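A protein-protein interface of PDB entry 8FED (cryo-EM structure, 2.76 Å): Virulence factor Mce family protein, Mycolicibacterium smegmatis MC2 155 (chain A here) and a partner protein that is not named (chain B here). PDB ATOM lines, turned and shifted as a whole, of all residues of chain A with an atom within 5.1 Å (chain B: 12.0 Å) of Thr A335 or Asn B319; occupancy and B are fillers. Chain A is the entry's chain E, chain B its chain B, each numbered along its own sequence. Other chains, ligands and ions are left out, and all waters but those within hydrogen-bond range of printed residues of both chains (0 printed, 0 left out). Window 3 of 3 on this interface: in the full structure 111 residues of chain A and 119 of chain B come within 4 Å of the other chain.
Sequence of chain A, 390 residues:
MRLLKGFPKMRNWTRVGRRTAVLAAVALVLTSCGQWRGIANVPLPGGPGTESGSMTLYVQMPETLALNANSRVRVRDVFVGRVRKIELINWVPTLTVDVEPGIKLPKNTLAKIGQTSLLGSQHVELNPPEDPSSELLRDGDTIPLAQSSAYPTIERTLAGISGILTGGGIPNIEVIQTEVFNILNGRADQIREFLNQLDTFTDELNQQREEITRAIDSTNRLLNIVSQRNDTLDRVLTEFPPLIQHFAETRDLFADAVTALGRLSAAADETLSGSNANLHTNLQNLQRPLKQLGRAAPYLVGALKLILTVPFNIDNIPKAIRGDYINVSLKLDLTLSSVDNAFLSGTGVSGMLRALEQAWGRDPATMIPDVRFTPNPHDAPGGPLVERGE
Of the 10 printed residues of chain A, 4 touch a printed residue of chain B. Hydrophobic or aromatic side chains of chain A that line the printed part of chain B: Leu A334. Among the printed residues, no Asp or Glu carboxylate lies within 4 Å of a Lys or Arg side-chain nitrogen of the other chain.
Thr A335 touches just these residues of chain B: Lys B317 (3.6 Å) and Asn B319 (3.4 Å). Asn B319 touches just one residue of chain A: Thr A335. Of chain B, only Lys B317 comes within 4 Å of Asp A333. Ser A337 touches none of the printed residues of chain B. No residue of chain B comes within 4 Å of Val A339. Printed residues of chain A within 4 Å of Lys B317: Asp A333 (3.2 Å), Leu A334 (2.6 Å) and Thr A335 (3.6 Å). Of the printed residues of chain B, Arg A362 touches Val B327 (3.7 Å). Of the printed residues of chain A, Val B327 touches Arg A362 (3.7 Å).
O of Lys B317 sits at hydrogen-bond distance from N of Leu A334.
The guanidinium group (NH2) of Arg A362 is in hydrogen-bond range of the side-chain hydroxyl (OG) of Ser A337, 3.3 Å away. O of Thr A335 is in hydrogen-bond range of OG of Ser A338 (2.5 Å). OE2 of Glu A357 is in salt-bridge range of NE of Arg A362, 2.7 Å away. The backbone carbonyl oxygen of Asp A333 lies within hydrogen-bond range of the side-chain hydroxyl of Ser A338 (3.5 Å). O of Leu B318 is in hydrogen-bond range of N of Val B327.
Among the printed residues, pairs that only touch across the chains: Asp A333 with Lys B317 (3.2 Å), Thr A335 with Asn B319 (3.4 Å), Thr A335 with Lys B317 (3.6 Å) and Arg A362 with Val B327 (3.7 Å).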
ATOM      1  N   ASP A 333      14.770  -5.447  20.961  1.00  0.00           N
ATOM      2  CA  ASP A 333      15.004  -5.144  19.557  1.00  0.00           C
ATOM      3  C   ASP A 333      15.481  -6.398  18.836  1.00  0.00           C
ATOM      4  O   ASP A 333      16.415  -7.067  19.289  1.00  0.00           O
ATOM      5  CB  ASP A 333      16.014  -4.006  19.385  1.00  0.00           C
ATOM      6  CG  ASP A 333      17.377  -4.340  19.944  1.00  0.00           C
ATOM      7  OD1 ASP A 333      17.440  -4.975  21.013  1.00  0.00           O
ATOM      8  OD2 ASP A 333      18.385  -3.972  19.308  1.00  0.00           O
ATOM      9  N   LEU A 334      14.819  -6.720  17.726  1.00  0.00           N
ATOM     10  CA  LEU A 334      15.152  -7.879  16.907  1.00  0.00           C
ATOM     11  C   LEU A 334      15.533  -7.460  15.491  1.00  0.00           C
ATOM     12  O   LEU A 334      15.373  -8.231  14.543  1.00  0.00           O
ATOM     13  CB  LEU A 334      13.990  -8.870  16.885  1.00  0.00           C
ATOM     14  CG  LEU A 334      13.457  -9.290  18.256  1.00  0.00           C
ATOM     15  CD1 LEU A 334      12.329 -10.297  18.112  1.00  0.00           C
ATOM     16  CD2 LEU A 334      14.573  -9.854  19.116  1.00  0.00           C
ATOM     17  N   THR A 335      16.027  -6.235  15.339  1.00  0.00           N
ATOM     18  CA  THR A 335      16.468  -5.749  14.041  1.00  0.00           C
ATOM     19  C   THR A 335      17.695  -6.531  13.581  1.00  0.00           C
ATOM     20  O   THR A 335      18.478  -7.031  14.393  1.00  0.00           O
ATOM     21  CB  THR A 335      16.784  -4.253  14.121  1.00  0.00           C
ATOM     22  OG1 THR A 335      15.743  -3.588  14.845  1.00  0.00           O
ATOM     23  CG2 THR A 335      16.874  -3.635  12.733  1.00  0.00           C
ATOM     24  N   LEU A 336      17.848  -6.645  12.258  1.00  0.00           N
ATOM     25  CA  LEU A 336      18.945  -7.423  11.690  1.00  0.00           C
ATOM     26  C   LEU A 336      20.314  -6.893  12.097  1.00  0.00           C
ATOM     27  O   LEU A 336      21.281  -7.659  12.102  1.00  0.00           O
ATOM     28  CB  LEU A 336      18.834  -7.457  10.166  1.00  0.00           C
ATOM     29  CG  LEU A 336      17.569  -8.097   9.590  1.00  0.00           C
ATOM     30  CD1 LEU A 336      17.647  -8.171   8.075  1.00  0.00           C
ATOM     31  CD2 LEU A 336      17.336  -9.475  10.185  1.00  0.00           C
ATOM     32  N   SER A 337      20.420  -5.607  12.436  1.00  0.00           N
ATOM     33  CA  SER A 337      21.682  -5.082  12.950  1.00  0.00           C
ATOM     34  C   SER A 337      22.018  -5.701  14.301  1.00  0.00           C
ATOM     35  O   SER A 337      23.155  -6.134  14.535  1.00  0.00           O
ATOM     36  CB  SER A 337      21.609  -3.560  13.057  1.00  0.00           C
ATOM     37  OG  SER A 337      20.552  -3.163  13.912  1.00  0.00           O
ATOM     38  N   SER A 338      21.033  -5.754  15.202  1.00  0.00           N
ATOM     39  CA  SER A 338      21.251  -6.362  16.510  1.00  0.00           C
ATOM     40  C   SER A 338      21.554  -7.848  16.383  1.00  0.00           C
ATOM     41  O   SER A 338      22.410  -8.377  17.099  1.00  0.00           O
ATOM     42  CB  SER A 338      20.033  -6.136  17.403  1.00  0.00           C
ATOM     43  OG  SER A 338      18.880  -6.752  16.855  1.00  0.00           O
ATOM     44  N   VAL A 339      20.855  -8.538  15.480  1.00  0.00           N
ATOM     45  CA  VAL A 339      21.105  -9.961  15.267  1.00  0.00           C
ATOM     46  C   VAL A 339      22.508 -10.183  14.718  1.00  0.00           C
ATOM     47  O   VAL A 339      23.220 -11.098  15.149  1.00  0.00           O
ATOM     48  CB  VAL A 339      20.030 -10.554  14.337  1.00  0.00           C
ATOM     49  CG1 VAL A 339      20.362 -11.992  13.981  1.00  0.00           C
ATOM     50  CG2 VAL A 339      18.666 -10.471  14.996  1.00  0.00           C
ATOM     51  N   ASP A 340      22.928  -9.353  13.761  1.00  0.00           N
ATOM     52  CA  ASP A 340      24.254  -9.511  13.174  1.00  0.00           C
ATOM     53  C   ASP A 340      25.349  -9.243  14.196  1.00  0.00           C
ATOM     54  O   ASP A 340      26.365  -9.947  14.222  1.00  0.00           O
ATOM     55  CB  ASP A 340      24.422  -8.587  11.973  1.00  0.00           C
ATOM     56  CG  ASP A 340      25.763  -8.768  11.295  1.00  0.00           C
ATOM     57  OD1 ASP A 340      25.981  -9.843  10.699  1.00  0.00           O
ATOM     58  OD2 ASP A 340      26.601  -7.846  11.361  1.00  0.00           O
ATOM     59  N   GLU A 357      20.319  -5.429   5.661  1.00  0.00           N
ATOM     60  CA  GLU A 357      19.656  -4.285   6.278  1.00  0.00           C
ATOM     61  C   GLU A 357      20.154  -2.973   5.686  1.00  0.00           C
ATOM     62  O   GLU A 357      19.364  -2.047   5.468  1.00  0.00           O
ATOM     63  CB  GLU A 357      19.868  -4.303   7.791  1.00  0.00           C
ATOM     64  CG  GLU A 357      19.296  -3.090   8.505  1.00  0.00           C
ATOM     65  CD  GLU A 357      19.457  -3.162  10.008  1.00  0.00           C
ATOM     66  OE1 GLU A 357      19.612  -4.282  10.534  1.00  0.00           O
ATOM     67  OE2 GLU A 357      19.428  -2.101  10.664  1.00  0.00           O
ATOM     68  N   ARG A 362      17.049   1.364   6.072  1.00  0.00           N
ATOM     69  CA  ARG A 362      17.765   1.761   7.275  1.00  0.00           C
ATOM     70  C   ARG A 362      19.070   2.467   6.921  1.00  0.00           C
ATOM     71  O   ARG A 362      19.675   2.222   5.874  1.00  0.00           O
ATOM     72  CB  ARG A 362      18.040   0.546   8.158  1.00  0.00           C
ATOM     73  CG  ARG A 362      16.797  -0.013   8.834  1.00  0.00           C
ATOM     74  CD  ARG A 362      16.684   0.454  10.276  1.00  0.00           C
ATOM     75  NE  ARG A 362      17.771  -0.059  11.101  1.00  0.00           N
ATOM     76  CZ  ARG A 362      17.866   0.122  12.411  1.00  0.00           C
ATOM     77  NH1 ARG A 362      16.957   0.809  13.082  1.00  0.00           N
ATOM     78  NH2 ARG A 362      18.900  -0.402  13.065  1.00  0.00           N
ATOM     79  N   THR B 315       8.477  -3.615  25.372  1.00  0.00           N
ATOM     80  CA  THR B 315       8.037  -3.430  24.000  1.00  0.00           C
ATOM     81  C   THR B 315       9.038  -4.080  23.055  1.00  0.00           C
ATOM     82  O   THR B 315      10.217  -4.230  23.385  1.00  0.00           O
ATOM     83  CB  THR B 315       7.897  -1.941  23.662  1.00  0.00           C
ATOM     84  OG1 THR B 315       7.718  -1.782  22.250  1.00  0.00           O
ATOM     85  CG2 THR B 315       9.136  -1.182  24.100  1.00  0.00           C
ATOM     86  N   LEU B 316       8.557  -4.459  21.874  1.00  0.00           N
ATOM     87  CA  LEU B 316       9.356  -5.144  20.864  1.00  0.00           C
ATOM     88  C   LEU B 316       9.670  -4.208  19.706  1.00  0.00           C
ATOM     89  O   LEU B 316       8.773  -3.545  19.176  1.00  0.00           O
ATOM     90  CB  LEU B 316       8.651  -6.402  20.354  1.00  0.00           C
ATOM     91  CG  LEU B 316       9.007  -7.712  21.063  1.00  0.00           C
ATOM     92  CD1 LEU B 316       8.759  -7.642  22.558  1.00  0.00           C
ATOM     93  CD2 LEU B 316       8.238  -8.872  20.444  1.00  0.00           C
ATOM     94  N   LYS B 317      10.941  -4.161  19.317  1.00  0.00           N
ATOM     95  CA  LYS B 317      11.402  -3.381  18.176  1.00  0.00           C
ATOM     96  C   LYS B 317      11.845  -4.341  17.080  1.00  0.00           C
ATOM     97  O   LYS B 317      12.722  -5.181  17.304  1.00  0.00           O
ATOM     98  CB  LYS B 317      12.549  -2.455  18.578  1.00  0.00           C
ATOM     99  CG  LYS B 317      13.315  -1.865  17.408  1.00  0.00           C
ATOM    100  CD  LYS B 317      14.482  -1.020  17.890  1.00  0.00           C
ATOM    101  CE  LYS B 317      15.306  -0.494  16.731  1.00  0.00           C
ATOM    102  NZ  LYS B 317      16.477   0.294  17.201  1.00  0.00           N
ATOM    103  N   LEU B 318      11.241  -4.219  15.900  1.00  0.00           N
ATOM    104  CA  LEU B 318      11.558  -5.116  14.796  1.00  0.00           C
ATOM    105  C   LEU B 318      11.151  -4.464  13.484  1.00  0.00           C
ATOM    106  O   LEU B 318      10.341  -3.534  13.454  1.00  0.00           O
ATOM    107  CB  LEU B 318      10.872  -6.478  14.971  1.00  0.00           C
ATOM    108  CG  LEU B 318       9.388  -6.524  15.358  1.00  0.00           C
ATOM    109  CD1 LEU B 318       8.465  -6.397  14.152  1.00  0.00           C
ATOM    110  CD2 LEU B 318       9.083  -7.798  16.129  1.00  0.00           C
ATOM    111  N   ASN B 319      11.726  -4.970  12.398  1.00  0.00           N
ATOM    112  CA  ASN B 319      11.414  -4.472  11.064  1.00  0.00           C
ATOM    113  C   ASN B 319      10.641  -5.506  10.252  1.00  0.00           C
ATOM    114  O   ASN B 319       9.499  -5.832  10.572  1.00  0.00           O
ATOM    115  CB  ASN B 319      12.694  -4.065  10.328  1.00  0.00           C
ATOM    116  CG  ASN B 319      13.780  -5.121  10.410  1.00  0.00           C
ATOM    117  OD1 ASN B 319      13.523  -6.271  10.763  1.00  0.00           O
ATOM    118  ND2 ASN B 319      15.005  -4.731  10.081  1.00  0.00           N
ATOM    119  N   VAL B 327      10.670  -1.227  11.072  1.00  0.00           N
ATOM    120  CA  VAL B 327      11.385  -0.565  12.153  1.00  0.00           C
ATOM    121  C   VAL B 327      10.382  -0.175  13.233  1.00  0.00           C
ATOM    122  O   VAL B 327      10.723   0.494  14.211  1.00  0.00           O
ATOM    123  CB  VAL B 327      12.175   0.655  11.627  1.00  0.00           C
ATOM    124  CG1 VAL B 327      11.248   1.843  11.381  1.00  0.00           C
ATOM    125  CG2 VAL B 327      13.327   1.014  12.565  1.00  0.00           C
ATOM    126  N   ARG B 328       9.139  -0.619  13.052  1.00  0.00           N
ATOM    127  CA  ARG B 328       8.077  -0.293  13.996  1.00  0.00           C
ATOM    128  C   ARG B 328       8.381  -0.869  15.372  1.00  0.00           C
ATOM    129  O   ARG B 328       8.926  -1.968  15.501  1.00  0.00           O
ATOM    130  CB  ARG B 328       6.735  -0.821  13.490  1.00  0.00           C
ATOM    131  CG  ARG B 328       6.715  -2.318  13.221  1.00  0.00           C
ATOM    132  CD  ARG B 328       5.296  -2.855  13.167  1.00  0.00           C
ATOM    133  NE  ARG B 328       5.268  -4.293  12.936  1.00  0.00           N
ATOM    134  CZ  ARG B 328       4.179  -5.045  13.021  1.00  0.00           C
ATOM    135  NH1 ARG B 328       3.006  -4.528  13.342  1.00  0.00           N
ATOM    136  NH2 ARG B 328       4.272  -6.350  12.779  1.00  0.00           N
ATOM    137  N   THR B 329       8.035  -0.110  16.406  1.00  0.00           N
ATOM    138  CA  THR B 329       8.187  -0.544  17.788  1.00  0.00           C
ATOM    139  C   THR B 329       6.810  -0.911  18.325  1.00  0.00           C
ATOM    140  O   THR B 329       5.942  -0.044  18.473  1.00  0.00           O
ATOM    141  CB  THR B 329       8.839   0.543  18.640  1.00  0.00           C
ATOM    142  OG1 THR B 329       8.050   1.739  18.579  1.00  0.00           O
ATOM    143  CG2 THR B 329      10.244   0.841  18.142  1.00  0.00           C
ATOM    144  N   VAL B 330       6.612  -2.191  18.621  1.00  0.00           N
ATOM    145  CA  VAL B 330       5.331  -2.704  19.087  1.00  0.00           C
ATOM    146  C   VAL B 330       5.370  -2.737  20.606  1.00  0.00           C
ATOM    147  O   VAL B 330       6.286  -3.320  21.198  1.00  0.00           O
ATOM    148  CB  VAL B 330       5.045  -4.102  18.512  1.00  0.00           C
ATOM    149  CG1 VAL B 330       3.709  -4.620  19.021  1.00  0.00           C
ATOM    150  CG2 VAL B 330       5.064  -4.064  16.993  1.00  0.00           C
ATOM    151  N   ARG B 331       4.376  -2.120  21.236  1.00  0.00           N
ATOM    152  CA  ARG B 331       4.300  -2.065  22.687  1.00  0.00           C
ATOM    153  C   ARG B 331       3.476  -3.235  23.205  1.00  0.00           C
ATOM    154  O   ARG B 331       2.372  -3.492  22.712  1.00  0.00           O
ATOM    155  CB  ARG B 331       3.691  -0.733  23.133  1.00  0.00           C
ATOM    156  CG  ARG B 331       3.517  -0.549  24.639  1.00  0.00           C
ATOM    157  CD  ARG B 331       2.113  -0.913  25.137  1.00  0.00           C
ATOM    158  NE  ARG B 331       1.053  -0.188  24.444  1.00  0.00           N
ATOM    159  CZ  ARG B 331       0.302  -0.700  23.478  1.00  0.00           C
ATOM    160  NH1 ARG B 331       0.465  -1.945  23.060  1.00  0.00           N
ATOM    161  NH2 ARG B 331      -0.637   0.058  22.917  1.00  0.00           N
